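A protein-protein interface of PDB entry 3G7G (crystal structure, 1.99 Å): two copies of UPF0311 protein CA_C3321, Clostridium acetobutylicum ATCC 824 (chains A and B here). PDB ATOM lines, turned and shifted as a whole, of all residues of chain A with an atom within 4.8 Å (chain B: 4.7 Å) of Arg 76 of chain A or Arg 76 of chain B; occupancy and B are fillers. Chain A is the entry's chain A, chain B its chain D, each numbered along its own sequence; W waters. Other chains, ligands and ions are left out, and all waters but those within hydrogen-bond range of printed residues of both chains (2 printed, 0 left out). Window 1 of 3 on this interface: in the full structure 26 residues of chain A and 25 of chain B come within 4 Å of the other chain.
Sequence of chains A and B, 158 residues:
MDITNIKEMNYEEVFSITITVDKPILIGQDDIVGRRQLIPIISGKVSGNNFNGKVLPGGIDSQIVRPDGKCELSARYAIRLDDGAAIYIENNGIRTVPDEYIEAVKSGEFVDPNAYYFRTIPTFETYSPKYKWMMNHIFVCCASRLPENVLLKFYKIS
OG of Ser 62 of chain A lies within hydrogen-bond range of OH of Tyr 88 of chain B (2.9 Å).
The guanidinium group (NH2) of Arg 76 of chain B lies within salt-bridge range of the side-chain carboxylate (OE2) of Glu 90 of chain A (3.7 Å).
The side-chain hydroxyl of Ser 74 of chain A sits at hydrogen-bond distance from the guanidinium group of Arg 76 of chain B, at 2.9 Å.
The side-chain hydroxyl (OG) of Ser 62 of chain B lies within hydrogen-bond range of the side-chain hydroxyl (OH) of Tyr 88 of chain A, at 2.8 Å.
OG of Ser 74 of chain B is in hydrogen-bond range of NH2 of Arg 76 of chain A (2.9 Å).
The backbone carbonyl oxygen (O) of Ile 60 of chain A lies within hydrogen-bond range of the backbone NH (N) of Arg 76 of chain A, at 3.0 Å.
The backbone NH (N) of Ser 62 of chain A is in hydrogen-bond range of the backbone carbonyl oxygen (O) of Ser 74 of chain A.
N of Arg 76 of chain B sits at hydrogen-bond distance from O of Ile 60 of chain B (3.0 Å).
N of Ser 74 of chain B is in hydrogen-bond range of O of Ser 62 of chain B (2.9 Å).
OE2 of Glu 90 of chain A is in salt-bridge range of NE of Arg 76 of chain A, 3.0 Å away.
The side-chain carboxylate of Glu 90 of chain A sits at hydrogen-bond distance from the side-chain hydroxyl of Ser 74 of chain A.
Ile 60 of chain B touches Gly 58 of chain A (CD1 to O, 3.4 Å).
Ile 60 of chain A touches Gly 58 of chain B (CG1 to O, 3.4 Å).
CG1 of Ile 60 of chain B touches CG1 of Ile 60 of chain A, at 3.99 Å.
CB of Ser 62 of chain A touches NH1 of Arg 76 of chain B, at 3.97 Å.
Arg 76 of chain A touches Ser 62 of chain B.
CZ of Arg 76 of chain A touches NE of Arg 76 of chain B, 3.5 Å away.
Of chain B, only Ser 62 (3.97 Å), Ser 74 (2.9 Å) and Arg 76 (3.5 Å) come within 4 Å of Arg 76 of chain A.
Arg 76 of chain B touches four residues of chain A.
Of the printed residues of chain B, Ser 62 of chain A touches Arg 76 and Tyr 88.
Printed residues of chain A within 4 Å of Gly 58 of chain B: Ile 60.
Of the printed residues of chain B, Ile 60 of chain A touches Gly 58 (3.4 Å) and Ile 60 (3.99 Å).
Printed residues of chain B within 4 Å of Glu 90 of chain A: Arg 76.
Printed residues of chain B within 4 Å of Gly 58 of chain A: Ile 60.
Gly 59 of chain A touches none of the printed residues of chain B.
The nearest printed residue of chain B that does not touch Tyr 88 of chain A is Ser 74 of chain B (6.7 Å).
Of the 11 printed residues of chain A, 7 touch a printed residue of chain B.
Hydrophobic or aromatic side chains of chain A within 4 Å of the printed part of chain B: Ile 60 and Tyr 88.
Along chain A the printed residues that touch a printed residue of chain B span positions 58 to 90.
Of the 11 printed residues of chain B, 6 touch a printed residue of chain A.
Printed residues of chain B that touch a printed residue of chain A: Gly 58, Ile 60, Ser 62, Ser 74, Arg 76 and Tyr 88.
Hydrophobic or aromatic side chains of chain B within 4 Å of the printed part of chain A: Ile 60 and Tyr 88.
Among the printed residues, Asp or Glu carboxylates within 4 Å of a Lys or Arg side-chain nitrogen of the other chain: Glu 90 of chain A with Arg 76 of chain B.
Gly 58 of chain A touches Ile 60 of chain B, and with the chains exchanged Ile 60 of chain A touches Gly 58 of chain B.
Ile 60 of chain B touches its own counterpart, Ile 60 of chain A.
Ser 74 of chain A touches Arg 76 of chain B, and with the chains exchanged Arg 76 of chain A touches Ser 74 of chain B.
Arg 76 of chain B touches its own counterpart, Arg 76 of chain A.
Positions printed for both chains: 58, 59, 60, 62, 74, 75, 76, 77, 88, 89 and 90.
Water W2 lies within hydrogen-bond range of the guanidinium group (NH1) of Arg 76 of chain A (2.7 Å), the backbone carbonyl oxygen (O) of Ile 60 of chain B (3.0 Å) and the backbone carbonyl oxygen (O) of Ser 74 of chain B (3.5 Å).
Water W1 lies within hydrogen-bond range of NH1 of Arg 76 of chain B (2.7 Å), O of Ile 60 of chain A (3.0 Å) and O of Ser 74 of chain A (3.4 Å).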
ATOM      1  N   GLY A  58      25.716 -25.437   3.980  1.00  0.00           N
ATOM      2  CA  GLY A  58      24.409 -25.376   3.314  1.00  0.00           C
ATOM      3  C   GLY A  58      23.384 -26.400   3.746  1.00  0.00           C
ATOM      4  O   GLY A  58      22.286 -26.400   3.236  1.00  0.00           O
ATOM      5  N   GLY A  59      23.766 -27.270   4.678  1.00  0.00           N
ATOM      6  CA  GLY A  59      22.959 -28.408   5.076  1.00  0.00           C
ATOM      7  C   GLY A  59      21.867 -28.043   6.054  1.00  0.00           C
ATOM      8  O   GLY A  59      22.087 -27.351   7.053  1.00  0.00           O
ATOM      9  N   ILE A  60      20.668 -28.508   5.753  1.00  0.00           N
ATOM     10  CA  ILE A  60      19.519 -28.325   6.616  1.00  0.00           C
ATOM     11  C   ILE A  60      18.715 -29.628   6.680  1.00  0.00           C
ATOM     12  O   ILE A  60      18.477 -30.254   5.643  1.00  0.00           O
ATOM     13  CB  ILE A  60      18.604 -27.233   6.057  1.00  0.00           C
ATOM     14  CG1 ILE A  60      19.246 -25.856   6.266  1.00  0.00           C
ATOM     15  CG2 ILE A  60      17.227 -27.299   6.717  1.00  0.00           C
ATOM     16  CD1 ILE A  60      19.212 -25.374   7.746  1.00  0.00           C
ATOM     17  N   SER A  62      15.000 -30.536   7.428  1.00  0.00           N
ATOM     18  CA  SER A  62      13.651 -30.087   7.632  1.00  0.00           C
ATOM     19  C   SER A  62      12.842 -31.224   8.266  1.00  0.00           C
ATOM     20  O   SER A  62      12.724 -32.298   7.697  1.00  0.00           O
ATOM     21  CB  SER A  62      13.033 -29.657   6.331  1.00  0.00           C
ATOM     22  OG  SER A  62      11.782 -29.081   6.586  1.00  0.00           O
ATOM     23  N   SER A  74      13.662 -34.816   6.575  1.00  0.00           N
ATOM     24  CA  SER A  74      14.165 -34.656   5.209  1.00  0.00           C
ATOM     25  C   SER A  74      15.349 -33.716   5.202  1.00  0.00           C
ATOM     26  O   SER A  74      15.190 -32.484   5.310  1.00  0.00           O
ATOM     27  CB  SER A  74      13.060 -34.172   4.279  1.00  0.00           C
ATOM     28  OG  SER A  74      13.500 -34.163   2.901  1.00  0.00           O
ATOM     29  N   ALA A  75      16.536 -34.282   5.087  1.00  0.00           N
ATOM     30  CA  ALA A  75      17.815 -33.516   5.098  1.00  0.00           C
ATOM     31  C   ALA A  75      18.432 -33.353   3.714  1.00  0.00           C
ATOM     32  O   ALA A  75      18.382 -34.265   2.908  1.00  0.00           O
ATOM     33  CB  ALA A  75      18.866 -34.174   6.071  1.00  0.00           C
ATOM     34  N   ARG A  76      18.915 -32.152   3.401  1.00  0.00           N
ATOM     35  CA  ARG A  76      19.625 -31.918   2.171  1.00  0.00           C
ATOM     36  C   ARG A  76      20.932 -31.285   2.519  1.00  0.00           C
ATOM     37  O   ARG A  76      20.961 -30.158   3.072  1.00  0.00           O
ATOM     38  CB  ARG A  76      18.884 -30.956   1.272  1.00  0.00           C
ATOM     39  CG  ARG A  76      17.529 -31.412   0.857  1.00  0.00           C
ATOM     40  CD  ARG A  76      16.841 -30.295   0.117  1.00  0.00           C
ATOM     41  NE  ARG A  76      15.711 -30.791  -0.624  1.00  0.00           N
ATOM     42  CZ  ARG A  76      14.885 -30.042  -1.321  1.00  0.00           C
ATOM     43  NH1 ARG A  76      15.058 -28.747  -1.361  1.00  0.00           N
ATOM     44  NH2 ARG A  76      13.883 -30.603  -1.986  1.00  0.00           N
ATOM     45  N   TYR A  77      22.003 -31.989   2.167  1.00  0.00           N
ATOM     46  CA  TYR A  77      23.361 -31.552   2.406  1.00  0.00           C
ATOM     47  C   TYR A  77      24.312 -32.302   1.475  1.00  0.00           C
ATOM     48  O   TYR A  77      23.879 -33.132   0.679  1.00  0.00           O
ATOM     49  CB  TYR A  77      23.721 -31.771   3.873  1.00  0.00           C
ATOM     50  CG  TYR A  77      23.631 -33.195   4.360  1.00  0.00           C
ATOM     51  CD1 TYR A  77      24.758 -34.001   4.435  1.00  0.00           C
ATOM     52  CD2 TYR A  77      22.432 -33.719   4.799  1.00  0.00           C
ATOM     53  CE1 TYR A  77      24.665 -35.304   4.904  1.00  0.00           C
ATOM     54  CE2 TYR A  77      22.330 -35.024   5.237  1.00  0.00           C
ATOM     55  CZ  TYR A  77      23.447 -35.811   5.303  1.00  0.00           C
ATOM     56  OH  TYR A  77      23.332 -37.114   5.773  1.00  0.00           O
ATOM     57  N   TYR A  88      25.974 -35.174  -3.160  1.00  0.00           N
ATOM     58  CA  TYR A  88      24.811 -34.482  -2.684  1.00  0.00           C
ATOM     59  C   TYR A  88      23.807 -35.519  -2.178  1.00  0.00           C
ATOM     60  O   TYR A  88      23.482 -36.500  -2.873  1.00  0.00           O
ATOM     61  CB  TYR A  88      24.227 -33.663  -3.816  1.00  0.00           C
ATOM     62  CG  TYR A  88      22.927 -33.048  -3.468  1.00  0.00           C
ATOM     63  CD1 TYR A  88      22.840 -32.088  -2.453  1.00  0.00           C
ATOM     64  CD2 TYR A  88      21.769 -33.422  -4.130  1.00  0.00           C
ATOM     65  CE1 TYR A  88      21.613 -31.518  -2.106  1.00  0.00           C
ATOM     66  CE2 TYR A  88      20.557 -32.846  -3.805  1.00  0.00           C
ATOM     67  CZ  TYR A  88      20.484 -31.910  -2.783  1.00  0.00           C
ATOM     68  OH  TYR A  88      19.276 -31.338  -2.475  1.00  0.00           O
ATOM     69  N   ILE A  89      23.328 -35.305  -0.968  1.00  0.00           N
ATOM     70  CA  ILE A  89      22.534 -36.290  -0.246  1.00  0.00           C
ATOM     71  C   ILE A  89      21.176 -35.697   0.074  1.00  0.00           C
ATOM     72  O   ILE A  89      21.125 -34.600   0.583  1.00  0.00           O
ATOM     73  CB  ILE A  89      23.201 -36.655   1.103  1.00  0.00           C
ATOM     74  CG1 ILE A  89      24.631 -37.076   0.864  1.00  0.00           C
ATOM     75  CG2 ILE A  89      22.429 -37.778   1.852  1.00  0.00           C
ATOM     76  CD1 ILE A  89      25.270 -37.706   2.017  1.00  0.00           C
ATOM     77  N   GLU A  90      20.112 -36.407  -0.297  1.00  0.00           N
ATOM     78  CA  GLU A  90      18.759 -36.177   0.192  1.00  0.00           C
ATOM     79  C   GLU A  90      18.424 -37.390   1.049  1.00  0.00           C
ATOM     80  O   GLU A  90      18.378 -38.493   0.525  1.00  0.00           O
ATOM     81  CB  GLU A  90      17.800 -36.097  -0.977  1.00  0.00           C
ATOM     82  CG  GLU A  90      17.242 -34.761  -1.278  1.00  0.00           C
ATOM     83  CD  GLU A  90      16.000 -34.457  -0.405  1.00  0.00           C
ATOM     84  OE1 GLU A  90      15.950 -34.972   0.755  1.00  0.00           O
ATOM     85  OE2 GLU A  90      15.095 -33.719  -0.881  1.00  0.00           O
ATOM     86  N   GLY B  58      17.516 -20.296   8.029  1.00  0.00           N
ATOM     87  CA  GLY B  58      17.487 -21.719   7.662  1.00  0.00           C
ATOM     88  C   GLY B  58      17.179 -22.047   6.226  1.00  0.00           C
ATOM     89  O   GLY B  58      17.124 -23.210   5.892  1.00  0.00           O
ATOM     90  N   GLY B  59      16.974 -21.019   5.401  1.00  0.00           N
ATOM     91  CA  GLY B  59      16.477 -21.160   4.041  1.00  0.00           C
ATOM     92  C   GLY B  59      17.583 -21.506   3.052  1.00  0.00           C
ATOM     93  O   GLY B  59      18.675 -20.928   3.074  1.00  0.00           O
ATOM     94  N   ILE B  60      17.288 -22.476   2.195  1.00  0.00           N
ATOM     95  CA  ILE B  60      18.209 -22.949   1.164  1.00  0.00           C
ATOM     96  C   ILE B  60      17.409 -23.229  -0.098  1.00  0.00           C
ATOM     97  O   ILE B  60      16.357 -23.880  -0.016  1.00  0.00           O
ATOM     98  CB  ILE B  60      18.857 -24.255   1.607  1.00  0.00           C
ATOM     99  CG1 ILE B  60      19.820 -23.986   2.793  1.00  0.00           C
ATOM    100  CG2 ILE B  60      19.582 -24.937   0.402  1.00  0.00           C
ATOM    101  CD1 ILE B  60      21.130 -23.294   2.403  1.00  0.00           C
ATOM    102  N   SER B  62      17.958 -25.479  -3.208  1.00  0.00           N
ATOM    103  CA  SER B  62      18.730 -26.505  -3.853  1.00  0.00           C
ATOM    104  C   SER B  62      18.384 -26.500  -5.354  1.00  0.00           C
ATOM    105  O   SER B  62      17.222 -26.684  -5.748  1.00  0.00           O
ATOM    106  CB  SER B  62      18.453 -27.856  -3.220  1.00  0.00           C
ATOM    107  OG  SER B  62      19.316 -28.826  -3.733  1.00  0.00           O
ATOM    108  N   SER B  74      14.446 -26.056  -6.082  1.00  0.00           N
ATOM    109  CA  SER B  74      13.660 -26.494  -4.932  1.00  0.00           C
ATOM    110  C   SER B  74      14.090 -25.746  -3.690  1.00  0.00           C
ATOM    111  O   SER B  74      15.097 -26.082  -3.106  1.00  0.00           O
ATOM    112  CB  SER B  74      13.805 -28.010  -4.748  1.00  0.00           C
ATOM    113  OG  SER B  74      12.884 -28.502  -3.783  1.00  0.00           O
ATOM    114  N   ALA B  75      13.320 -24.743  -3.267  1.00  0.00           N
ATOM    115  CA  ALA B  75      13.622 -23.958  -2.043  1.00  0.00           C
ATOM    116  C   ALA B  75      12.821 -24.374  -0.809  1.00  0.00           C
ATOM    117  O   ALA B  75      11.643 -24.616  -0.915  1.00  0.00           O
ATOM    118  CB  ALA B  75      13.422 -22.421  -2.311  1.00  0.00           C
ATOM    119  N   ARG B  76      13.474 -24.487   0.354  1.00  0.00           N
ATOM    120  CA  ARG B  76      12.779 -24.693   1.603  1.00  0.00           C
ATOM    121  C   ARG B  76      13.127 -23.567   2.548  1.00  0.00           C
ATOM    122  O   ARG B  76      14.286 -23.370   2.893  1.00  0.00           O
ATOM    123  CB  ARG B  76      13.159 -26.001   2.252  1.00  0.00           C
ATOM    124  CG  ARG B  76      12.861 -27.216   1.409  1.00  0.00           C
ATOM    125  CD  ARG B  76      13.467 -28.425   2.071  1.00  0.00           C
ATOM    126  NE  ARG B  76      12.901 -29.634   1.522  1.00  0.00           N
ATOM    127  CZ  ARG B  76      13.260 -30.852   1.890  1.00  0.00           C
ATOM    128  NH1 ARG B  76      14.182 -31.022   2.788  1.00  0.00           N
ATOM    129  NH2 ARG B  76      12.692 -31.901   1.344  1.00  0.00           N
ATOM    130  N   TYR B  77      12.113 -22.827   2.953  1.00  0.00           N
ATOM    131  CA  TYR B  77      12.305 -21.691   3.845  1.00  0.00           C
ATOM    132  C   TYR B  77      10.979 -21.307   4.477  1.00  0.00           C
ATOM    133  O   TYR B  77       9.931 -21.831   4.095  1.00  0.00           O
ATOM    134  CB  TYR B  77      12.923 -20.510   3.077  1.00  0.00           C
ATOM    135  CG  TYR B  77      12.118 -19.965   1.929  1.00  0.00           C
ATOM    136  CD1 TYR B  77      11.343 -18.808   2.076  1.00  0.00           C
ATOM    137  CD2 TYR B  77      12.176 -20.550   0.687  1.00  0.00           C
ATOM    138  CE1 TYR B  77      10.637 -18.295   1.010  1.00  0.00           C
ATOM    139  CE2 TYR B  77      11.457 -20.076  -0.355  1.00  0.00           C
ATOM    140  CZ  TYR B  77      10.709 -18.929  -0.203  1.00  0.00           C
ATOM    141  OH  TYR B  77      10.015 -18.474  -1.273  1.00  0.00           O
ATOM    142  N   TYR B  88       5.624 -22.111   6.333  1.00  0.00           N
ATOM    143  CA  TYR B  88       6.726 -22.893   5.812  1.00  0.00           C
ATOM    144  C   TYR B  88       6.466 -23.144   4.323  1.00  0.00           C
ATOM    145  O   TYR B  88       5.362 -23.511   3.926  1.00  0.00           O
ATOM    146  CB  TYR B  88       6.858 -24.176   6.608  1.00  0.00           C
ATOM    147  CG  TYR B  88       7.833 -25.138   6.010  1.00  0.00           C
ATOM    148  CD1 TYR B  88       9.202 -24.862   6.008  1.00  0.00           C
ATOM    149  CD2 TYR B  88       7.400 -26.322   5.429  1.00  0.00           C
ATOM    150  CE1 TYR B  88      10.115 -25.745   5.420  1.00  0.00           C
ATOM    151  CE2 TYR B  88       8.294 -27.201   4.876  1.00  0.00           C
ATOM    152  CZ  TYR B  88       9.646 -26.896   4.861  1.00  0.00           C
ATOM    153  OH  TYR B  88      10.533 -27.780   4.327  1.00  0.00           O
ATOM    154  N   ILE B  89       7.467 -22.886   3.502  1.00  0.00           N
ATOM    155  CA  ILE B  89       7.306 -22.835   2.068  1.00  0.00           C
ATOM    156  C   ILE B  89       8.247 -23.847   1.455  1.00  0.00           C
ATOM    157  O   ILE B  89       9.409 -23.806   1.757  1.00  0.00           O
ATOM    158  CB  ILE B  89       7.672 -21.418   1.513  1.00  0.00           C
ATOM    159  CG1 ILE B  89       6.773 -20.373   2.118  1.00  0.00           C
ATOM    160  CG2 ILE B  89       7.506 -21.345  -0.006  1.00  0.00           C
ATOM    161  CD1 ILE B  89       7.067 -18.974   1.677  1.00  0.00           C
ATOM    162  N   GLU B  90       7.745 -24.763   0.624  1.00  0.00           N
ATOM    163  CA  GLU B  90       8.610 -25.401  -0.340  1.00  0.00           C
ATOM    164  C   GLU B  90       8.202 -24.962  -1.730  1.00  0.00           C
ATOM    165  O   GLU B  90       7.078 -25.174  -2.131  1.00  0.00           O
ATOM    166  CB  GLU B  90       8.648 -26.915  -0.205  1.00  0.00           C
ATOM    167  CG  GLU B  90       9.882 -27.482  -1.025  1.00  0.00           C
ATOM    168  CD  GLU B  90       9.992 -28.987  -0.993  1.00  0.00           C
ATOM    169  OE1 GLU B  90      10.530 -29.501  -0.004  1.00  0.00           O
ATOM    170  OE2 GLU B  90       9.537 -29.639  -1.969  1.00  0.00           O
HETATM  171  O   HOH W   1      16.166 -29.542   3.950  1.00  0.00           O
HETATM  172  O   HOH W   2      16.405 -26.917   0.003  1.00  0.00           O
